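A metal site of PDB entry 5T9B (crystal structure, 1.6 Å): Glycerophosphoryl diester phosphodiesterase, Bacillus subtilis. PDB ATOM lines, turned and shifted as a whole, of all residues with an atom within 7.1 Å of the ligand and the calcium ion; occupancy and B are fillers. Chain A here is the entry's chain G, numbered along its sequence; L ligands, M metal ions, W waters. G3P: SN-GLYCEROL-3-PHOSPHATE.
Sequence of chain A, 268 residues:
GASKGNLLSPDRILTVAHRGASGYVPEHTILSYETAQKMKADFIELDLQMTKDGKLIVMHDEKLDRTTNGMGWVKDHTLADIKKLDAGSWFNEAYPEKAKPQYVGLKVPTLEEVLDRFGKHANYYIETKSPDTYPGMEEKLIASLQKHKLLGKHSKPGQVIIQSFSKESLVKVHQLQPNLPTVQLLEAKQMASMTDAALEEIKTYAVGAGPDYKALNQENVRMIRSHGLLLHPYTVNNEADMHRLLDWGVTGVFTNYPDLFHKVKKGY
OE1 of Gln 163 lies close to O1 of the ligand, 2.7 Å away.
The guanidinium group (NH2) of Arg 19 lies within salt-bridge range of an oxygen (O4P) of the ligand, 2.8 Å away.
O4P of the ligand sits at hydrogen-bond distance from NE2 of His 18.
NE2 of His 60 is in hydrogen-bond range of O2P of the ligand (2.8 Å).
OE2 of Glu 45 sits close to NE2 of Gln 163 (2.8 Å).
OE1 of Glu 45 is in hydrogen-bond range of N of Arg 19 (2.9 Å).
The guanidinium group (NE) of Arg 19 lies close to a ring nitrogen (NE2) of His 18 (3.5 Å).
NH2 of Arg 19 lies within hydrogen-bond range of NE2 of His 60 (3.2 Å).
The backbone NH (N) of His 28 is in hydrogen-bond range of the backbone carbonyl oxygen (O) of Arg 19.
A ring nitrogen (NE2) of His 18 lies close to the side-chain hydroxyl of Thr 235, at 3.3 Å.
O of Ser 164 sits at hydrogen-bond distance from N of Leu 185 (2.9 Å).
The backbone NH of Phe 254 sits at hydrogen-bond distance from the backbone carbonyl oxygen of Pro 233 (2.9 Å).
CD1 of Leu 185 touches O1 of the ligand (3.4 Å).
Tyr 234 touches the ligand (CD1 to O1P, 3.3 Å).
Phe 254 touches the ligand.
Hydrophobic or aromatic side chains that line the ligand: His 18, His 60, Leu 185, Tyr 234 and Phe 254.
Within 4 Å of the ligand: His 18, Arg 19, Glu 45, His 60, Glu 127, Gln 163, Leu 185, Tyr 234 and Phe 254.
Merely in contact with the calcium ion: Gln 163 (3.9 Å).
Of the 20 residues printed, 4 come within 4 Å of the calcium ion.
The nearest printed residue that does not touch the calcium ion is His 18 (4.7 Å).
The calcium ion is bound by an oxygen (O2) of the ligand (2.1 Å), the side-chain carboxylate of Glu 45 (2.3 Å), water W3 (2.3 Å), the side-chain carboxylate of Glu 127 (2.3 Å), the side-chain carboxylate of Asp 47 (2.4 Å), an oxygen (O1) of the ligand (2.5 Å) and water W6 (2.6 Å).
Water W6 lies within hydrogen-bond range of OD2 of Asp 47, OE1 of Glu 45, NE of Arg 19, NE2 of His 18 and O4P of the ligand.
Water W3 lies within hydrogen-bond range of an oxygen (O2P) of the ligand (2.8 Å), a ring nitrogen (NE2) of His 60 (3.4 Å) and the side-chain carboxylate of Glu 127 (3.4 Å).
Water W4 lies within hydrogen-bond range of an oxygen (O3P) of the ligand (2.7 Å) and the guanidinium group of Arg 19 (3.1 Å).
Water W2 lies within hydrogen-bond range of the side-chain hydroxyl (OG1) of Thr 235 and an oxygen (O3P) of the ligand.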
ATOM      1  N   HIS A  18     -17.775  14.219 -13.686  1.00  0.00           N
ATOM      2  CA  HIS A  18     -18.936  13.449 -13.247  1.00  0.00           C
ATOM      3  C   HIS A  18     -20.186  13.840 -14.035  1.00  0.00           C
ATOM      4  O   HIS A  18     -20.744  14.908 -13.839  1.00  0.00           O
ATOM      5  CB  HIS A  18     -19.123  13.702 -11.754  1.00  0.00           C
ATOM      6  CG  HIS A  18     -20.215  12.904 -11.111  1.00  0.00           C
ATOM      7  ND1 HIS A  18     -21.259  13.481 -10.437  1.00  0.00           N
ATOM      8  CD2 HIS A  18     -20.377  11.555 -10.983  1.00  0.00           C
ATOM      9  CE1 HIS A  18     -22.045  12.541  -9.944  1.00  0.00           C
ATOM     10  NE2 HIS A  18     -21.524  11.366 -10.253  1.00  0.00           N
ATOM     11  N   ARG A  19     -20.620  12.960 -14.921  1.00  0.00           N
ATOM     12  CA  ARG A  19     -21.730  13.279 -15.812  1.00  0.00           C
ATOM     13  C   ARG A  19     -21.445  14.534 -16.665  1.00  0.00           C
ATOM     14  O   ARG A  19     -22.355  15.258 -17.060  1.00  0.00           O
ATOM     15  CB  ARG A  19     -23.040  13.444 -15.003  1.00  0.00           C
ATOM     16  CG  ARG A  19     -23.180  12.457 -13.874  1.00  0.00           C
ATOM     17  CD  ARG A  19     -24.520  12.526 -13.193  1.00  0.00           C
ATOM     18  NE  ARG A  19     -24.502  11.751 -11.958  1.00  0.00           N
ATOM     19  CZ  ARG A  19     -25.382  11.869 -10.976  1.00  0.00           C
ATOM     20  NH1 ARG A  19     -26.372  12.747 -11.070  1.00  0.00           N
ATOM     21  NH2 ARG A  19     -25.238  11.149  -9.878  1.00  0.00           N
ATOM     22  N   HIS A  28     -25.055  14.632 -18.339  1.00  0.00           N
ATOM     23  CA  HIS A  28     -25.202  13.619 -19.389  1.00  0.00           C
ATOM     24  C   HIS A  28     -25.877  14.169 -20.633  1.00  0.00           C
ATOM     25  O   HIS A  28     -26.799  13.547 -21.201  1.00  0.00           O
ATOM     26  CB  HIS A  28     -25.960  12.403 -18.836  1.00  0.00           C
ATOM     27  CG  HIS A  28     -25.188  11.597 -17.837  1.00  0.00           C
ATOM     28  ND1 HIS A  28     -23.839  11.339 -17.962  1.00  0.00           N
ATOM     29  CD2 HIS A  28     -25.591  10.951 -16.712  1.00  0.00           C
ATOM     30  CE1 HIS A  28     -23.440  10.574 -16.962  1.00  0.00           C
ATOM     31  NE2 HIS A  28     -24.485  10.317 -16.193  1.00  0.00           N
ATOM     32  N   GLU A  45     -17.503  11.292 -17.953  1.00  0.00           N
ATOM     33  CA  GLU A  45     -18.087  10.145 -17.261  1.00  0.00           C
ATOM     34  C   GLU A  45     -19.531   9.879 -17.693  1.00  0.00           C
ATOM     35  O   GLU A  45     -20.370  10.782 -17.684  1.00  0.00           O
ATOM     36  CB  GLU A  45     -18.012  10.358 -15.732  1.00  0.00           C
ATOM     37  CG  GLU A  45     -18.305   9.092 -14.922  1.00  0.00           C
ATOM     38  CD  GLU A  45     -19.623   9.134 -14.157  1.00  0.00           C
ATOM     39  OE1 GLU A  45     -20.304  10.193 -14.164  1.00  0.00           O
ATOM     40  OE2 GLU A  45     -19.966   8.109 -13.547  1.00  0.00           O
ATOM     41  N   LEU A  46     -19.780   8.632 -18.092  1.00  0.00           N
ATOM     42  CA  LEU A  46     -21.066   8.199 -18.650  1.00  0.00           C
ATOM     43  C   LEU A  46     -21.708   7.104 -17.780  1.00  0.00           C
ATOM     44  O   LEU A  46     -21.025   6.178 -17.340  1.00  0.00           O
ATOM     45  CB  LEU A  46     -20.858   7.656 -20.069  1.00  0.00           C
ATOM     46  CG  LEU A  46     -20.639   8.603 -21.243  1.00  0.00           C
ATOM     47  CD1 LEU A  46     -19.387   9.453 -21.146  1.00  0.00           C
ATOM     48  CD2 LEU A  46     -20.586   7.774 -22.535  1.00  0.00           C
ATOM     49  N   ASP A  47     -23.021   7.208 -17.552  1.00  0.00           N
ATOM     50  CA  ASP A  47     -23.815   6.137 -16.940  1.00  0.00           C
ATOM     51  C   ASP A  47     -24.713   5.568 -18.031  1.00  0.00           C
ATOM     52  O   ASP A  47     -25.368   6.344 -18.707  1.00  0.00           O
ATOM     53  CB  ASP A  47     -24.680   6.621 -15.776  1.00  0.00           C
ATOM     54  CG  ASP A  47     -23.874   7.294 -14.675  1.00  0.00           C
ATOM     55  OD1 ASP A  47     -22.876   6.714 -14.180  1.00  0.00           O
ATOM     56  OD2 ASP A  47     -24.275   8.415 -14.291  1.00  0.00           O
ATOM     57  N   HIS A  60     -28.286   8.744 -15.663  1.00  0.00           N
ATOM     58  CA  HIS A  60     -27.865   8.246 -14.370  1.00  0.00           C
ATOM     59  C   HIS A  60     -28.910   7.321 -13.737  1.00  0.00           C
ATOM     60  O   HIS A  60     -28.575   6.240 -13.248  1.00  0.00           O
ATOM     61  CB  HIS A  60     -27.561   9.393 -13.400  1.00  0.00           C
ATOM     62  CG  HIS A  60     -27.212   8.925 -12.027  1.00  0.00           C
ATOM     63  ND1 HIS A  60     -28.144   8.831 -11.018  1.00  0.00           N
ATOM     64  CD2 HIS A  60     -26.056   8.431 -11.514  1.00  0.00           C
ATOM     65  CE1 HIS A  60     -27.572   8.351  -9.926  1.00  0.00           C
ATOM     66  NE2 HIS A  60     -26.307   8.113 -10.197  1.00  0.00           N
ATOM     67  N   TYR A 125     -15.185   7.369 -19.235  1.00  0.00           N
ATOM     68  CA  TYR A 125     -15.282   6.654 -17.968  1.00  0.00           C
ATOM     69  C   TYR A 125     -16.717   6.136 -17.873  1.00  0.00           C
ATOM     70  O   TYR A 125     -17.627   6.884 -17.539  1.00  0.00           O
ATOM     71  CB  TYR A 125     -14.924   7.589 -16.797  1.00  0.00           C
ATOM     72  CG  TYR A 125     -14.225   6.980 -15.597  1.00  0.00           C
ATOM     73  CD1 TYR A 125     -14.828   5.985 -14.832  1.00  0.00           C
ATOM     74  CD2 TYR A 125     -12.985   7.461 -15.186  1.00  0.00           C
ATOM     75  CE1 TYR A 125     -14.201   5.461 -13.714  1.00  0.00           C
ATOM     76  CE2 TYR A 125     -12.342   6.945 -14.068  1.00  0.00           C
ATOM     77  CZ  TYR A 125     -12.955   5.955 -13.331  1.00  0.00           C
ATOM     78  OH  TYR A 125     -12.330   5.448 -12.227  1.00  0.00           O
ATOM     79  N   ILE A 126     -16.924   4.859 -18.224  1.00  0.00           N
ATOM     80  CA  ILE A 126     -18.271   4.361 -18.555  1.00  0.00           C
ATOM     81  C   ILE A 126     -18.811   3.325 -17.559  1.00  0.00           C
ATOM     82  O   ILE A 126     -18.168   2.309 -17.303  1.00  0.00           O
ATOM     83  CB  ILE A 126     -18.288   3.752 -19.977  1.00  0.00           C
ATOM     84  CG1 ILE A 126     -17.753   4.758 -20.987  1.00  0.00           C
ATOM     85  CG2 ILE A 126     -19.708   3.331 -20.340  1.00  0.00           C
ATOM     86  CD1 ILE A 126     -17.664   4.181 -22.433  1.00  0.00           C
ATOM     87  N   GLU A 127     -19.993   3.600 -17.006  1.00  0.00           N
ATOM     88  CA  GLU A 127     -20.531   2.739 -15.952  1.00  0.00           C
ATOM     89  C   GLU A 127     -21.524   1.692 -16.467  1.00  0.00           C
ATOM     90  O   GLU A 127     -22.475   2.025 -17.149  1.00  0.00           O
ATOM     91  CB  GLU A 127     -21.235   3.562 -14.879  1.00  0.00           C
ATOM     92  CG  GLU A 127     -21.632   2.746 -13.664  1.00  0.00           C
ATOM     93  CD  GLU A 127     -21.998   3.609 -12.478  1.00  0.00           C
ATOM     94  OE1 GLU A 127     -21.439   4.729 -12.341  1.00  0.00           O
ATOM     95  OE2 GLU A 127     -22.858   3.185 -11.679  1.00  0.00           O
ATOM     96  N   GLN A 163     -16.395   1.248 -15.262  1.00  0.00           N
ATOM     97  CA  GLN A 163     -16.664   1.281 -13.834  1.00  0.00           C
ATOM     98  C   GLN A 163     -17.995   0.647 -13.530  1.00  0.00           C
ATOM     99  O   GLN A 163     -18.892   0.657 -14.366  1.00  0.00           O
ATOM    100  CB  GLN A 163     -16.652   2.738 -13.334  1.00  0.00           C
ATOM    101  CG  GLN A 163     -17.579   3.608 -14.187  1.00  0.00           C
ATOM    102  CD  GLN A 163     -17.897   4.941 -13.548  1.00  0.00           C
ATOM    103  OE1 GLN A 163     -17.619   5.153 -12.370  1.00  0.00           O
ATOM    104  NE2 GLN A 163     -18.480   5.839 -14.323  1.00  0.00           N
ATOM    105  N   SER A 164     -18.149   0.088 -12.331  1.00  0.00           N
ATOM    106  CA  SER A 164     -19.432  -0.460 -11.914  1.00  0.00           C
ATOM    107  C   SER A 164     -19.447  -0.725 -10.403  1.00  0.00           C
ATOM    108  O   SER A 164     -18.406  -1.009  -9.807  1.00  0.00           O
ATOM    109  CB  SER A 164     -19.734  -1.767 -12.674  1.00  0.00           C
ATOM    110  OG  SER A 164     -21.018  -2.267 -12.341  1.00  0.00           O
ATOM    111  N   PHE A 165     -20.625  -0.620  -9.789  1.00  0.00           N
ATOM    112  CA  PHE A 165     -20.802  -1.104  -8.419  1.00  0.00           C
ATOM    113  C   PHE A 165     -20.856  -2.627  -8.402  1.00  0.00           C
ATOM    114  O   PHE A 165     -20.671  -3.265  -7.353  1.00  0.00           O
ATOM    115  CB  PHE A 165     -22.074  -0.528  -7.790  1.00  0.00           C
ATOM    116  CG  PHE A 165     -21.972   0.915  -7.406  1.00  0.00           C
ATOM    117  CD1 PHE A 165     -21.580   1.276  -6.115  1.00  0.00           C
ATOM    118  CD2 PHE A 165     -22.279   1.918  -8.306  1.00  0.00           C
ATOM    119  CE1 PHE A 165     -21.485   2.618  -5.754  1.00  0.00           C
ATOM    120  CE2 PHE A 165     -22.187   3.255  -7.951  1.00  0.00           C
ATOM    121  CZ  PHE A 165     -21.790   3.605  -6.668  1.00  0.00           C
ATOM    122  N   LEU A 185     -16.522   0.412  -8.111  1.00  0.00           N
ATOM    123  CA  LEU A 185     -17.199   1.436  -7.341  1.00  0.00           C
ATOM    124  C   LEU A 185     -17.660   0.860  -5.994  1.00  0.00           C
ATOM    125  O   LEU A 185     -18.100  -0.281  -5.914  1.00  0.00           O
ATOM    126  CB  LEU A 185     -18.385   1.994  -8.121  1.00  0.00           C
ATOM    127  CG  LEU A 185     -18.029   2.648  -9.458  1.00  0.00           C
ATOM    128  CD1 LEU A 185     -19.286   3.090 -10.202  1.00  0.00           C
ATOM    129  CD2 LEU A 185     -17.074   3.833  -9.244  1.00  0.00           C
ATOM    130  N   GLY A 210     -13.270   3.148  -6.726  1.00  0.00           N
ATOM    131  CA  GLY A 210     -13.991   4.411  -6.680  1.00  0.00           C
ATOM    132  C   GLY A 210     -15.007   4.472  -5.553  1.00  0.00           C
ATOM    133  O   GLY A 210     -16.185   4.165  -5.765  1.00  0.00           O
ATOM    134  N   HIS A 232     -10.125   6.865  -7.079  1.00  0.00           N
ATOM    135  CA  HIS A 232     -10.930   7.973  -7.592  1.00  0.00           C
ATOM    136  C   HIS A 232     -12.226   8.100  -6.813  1.00  0.00           C
ATOM    137  O   HIS A 232     -13.240   7.509  -7.194  1.00  0.00           O
ATOM    138  CB  HIS A 232     -11.272   7.762  -9.080  1.00  0.00           C
ATOM    139  CG  HIS A 232     -10.076   7.576  -9.971  1.00  0.00           C
ATOM    140  ND1 HIS A 232     -10.165   6.948 -11.201  1.00  0.00           N
ATOM    141  CD2 HIS A 232      -8.783   7.959  -9.839  1.00  0.00           C
ATOM    142  CE1 HIS A 232      -8.975   6.931 -11.772  1.00  0.00           C
ATOM    143  NE2 HIS A 232      -8.120   7.539 -10.962  1.00  0.00           N
ATOM    144  N   PRO A 233     -12.217   8.841  -5.700  1.00  0.00           N
ATOM    145  CA  PRO A 233     -13.478   8.997  -4.963  1.00  0.00           C
ATOM    146  C   PRO A 233     -14.501   9.868  -5.672  1.00  0.00           C
ATOM    147  O   PRO A 233     -14.151  10.723  -6.489  1.00  0.00           O
ATOM    148  CB  PRO A 233     -13.042   9.661  -3.648  1.00  0.00           C
ATOM    149  CG  PRO A 233     -11.746  10.314  -3.965  1.00  0.00           C
ATOM    150  CD  PRO A 233     -11.087   9.490  -5.016  1.00  0.00           C
ATOM    151  N   TYR A 234     -15.773   9.633  -5.350  1.00  0.00           N
ATOM    152  CA  TYR A 234     -16.887  10.423  -5.846  1.00  0.00           C
ATOM    153  C   TYR A 234     -17.725  10.894  -4.669  1.00  0.00           C
ATOM    154  O   TYR A 234     -17.622  10.314  -3.589  1.00  0.00           O
ATOM    155  CB  TYR A 234     -17.747   9.571  -6.793  1.00  0.00           C
ATOM    156  CG  TYR A 234     -18.468   8.462  -6.056  1.00  0.00           C
ATOM    157  CD1 TYR A 234     -19.698   8.682  -5.432  1.00  0.00           C
ATOM    158  CD2 TYR A 234     -17.923   7.179  -5.985  1.00  0.00           C
ATOM    159  CE1 TYR A 234     -20.343   7.677  -4.738  1.00  0.00           C
ATOM    160  CE2 TYR A 234     -18.563   6.163  -5.284  1.00  0.00           C
ATOM    161  CZ  TYR A 234     -19.783   6.425  -4.674  1.00  0.00           C
ATOM    162  OH  TYR A 234     -20.428   5.420  -3.980  1.00  0.00           O
ATOM    163  N   THR A 235     -18.524  11.950  -4.829  1.00  0.00           N
ATOM    164  CA  THR A 235     -18.383  12.937  -5.888  1.00  0.00           C
ATOM    165  C   THR A 235     -17.810  14.184  -5.191  1.00  0.00           C
ATOM    166  O   THR A 235     -18.452  14.745  -4.300  1.00  0.00           O
ATOM    167  CB  THR A 235     -19.729  13.267  -6.576  1.00  0.00           C
ATOM    168  OG1 THR A 235     -20.194  12.100  -7.281  1.00  0.00           O
ATOM    169  CG2 THR A 235     -19.572  14.413  -7.569  1.00  0.00           C
ATOM    170  N   PHE A 254     -13.987  11.947  -9.094  1.00  0.00           N
ATOM    171  CA  PHE A 254     -15.168  12.319  -9.856  1.00  0.00           C
ATOM    172  C   PHE A 254     -15.670  13.651  -9.326  1.00  0.00           C
ATOM    173  O   PHE A 254     -15.913  13.767  -8.124  1.00  0.00           O
ATOM    174  CB  PHE A 254     -16.291  11.291  -9.746  1.00  0.00           C
ATOM    175  CG  PHE A 254     -15.934   9.914 -10.210  1.00  0.00           C
ATOM    176  CD1 PHE A 254     -15.217   9.034  -9.402  1.00  0.00           C
ATOM    177  CD2 PHE A 254     -16.385   9.457 -11.443  1.00  0.00           C
ATOM    178  CE1 PHE A 254     -14.922   7.753  -9.821  1.00  0.00           C
ATOM    179  CE2 PHE A 254     -16.094   8.169 -11.869  1.00  0.00           C
ATOM    180  CZ  PHE A 254     -15.361   7.320 -11.069  1.00  0.00           C
HETATM  181  O1  G3P L   1     -19.567   6.379 -10.883  1.00  0.00           O
HETATM  182  C1  G3P L   1     -19.133   7.339  -9.897  1.00  0.00           C
HETATM  183  C2  G3P L   1     -20.371   8.081  -9.485  1.00  0.00           C
HETATM  184  O2  G3P L   1     -21.083   8.426 -10.675  1.00  0.00           O
HETATM  185  C3  G3P L   1     -21.152   7.129  -8.589  1.00  0.00           C
HETATM  186  O1P G3P L   1     -21.945   7.808  -7.644  1.00  0.00           O
HETATM  187  O4P G3P L   1     -23.184   9.460  -9.145  1.00  0.00           O
HETATM  188  O2P G3P L   1     -24.224   7.282  -8.549  1.00  0.00           O
HETATM  189  O3P G3P L   1     -24.004   9.076  -6.847  1.00  0.00           O
HETATM  190  P   G3P L   1     -23.360   8.427  -8.044  1.00  0.00           P
HETATM  191 CA    CA M   1     -21.579   7.069 -12.231  1.00  0.00          CA
HETATM  192  O   HOH W   1     -24.189   8.157  -4.216  1.00  0.00           O
HETATM  193  O   HOH W   2     -22.504  11.260  -6.003  1.00  0.00           O
HETATM  194  O   HOH W   3     -23.537   6.462 -11.113  1.00  0.00           O
HETATM  195  O   HOH W   4     -26.305  10.367  -7.099  1.00  0.00           O
HETATM  196  O   HOH W   5     -25.866   5.446  -7.270  1.00  0.00           O
HETATM  197  O   HOH W   6     -22.532   9.431 -12.583  1.00  0.00           O
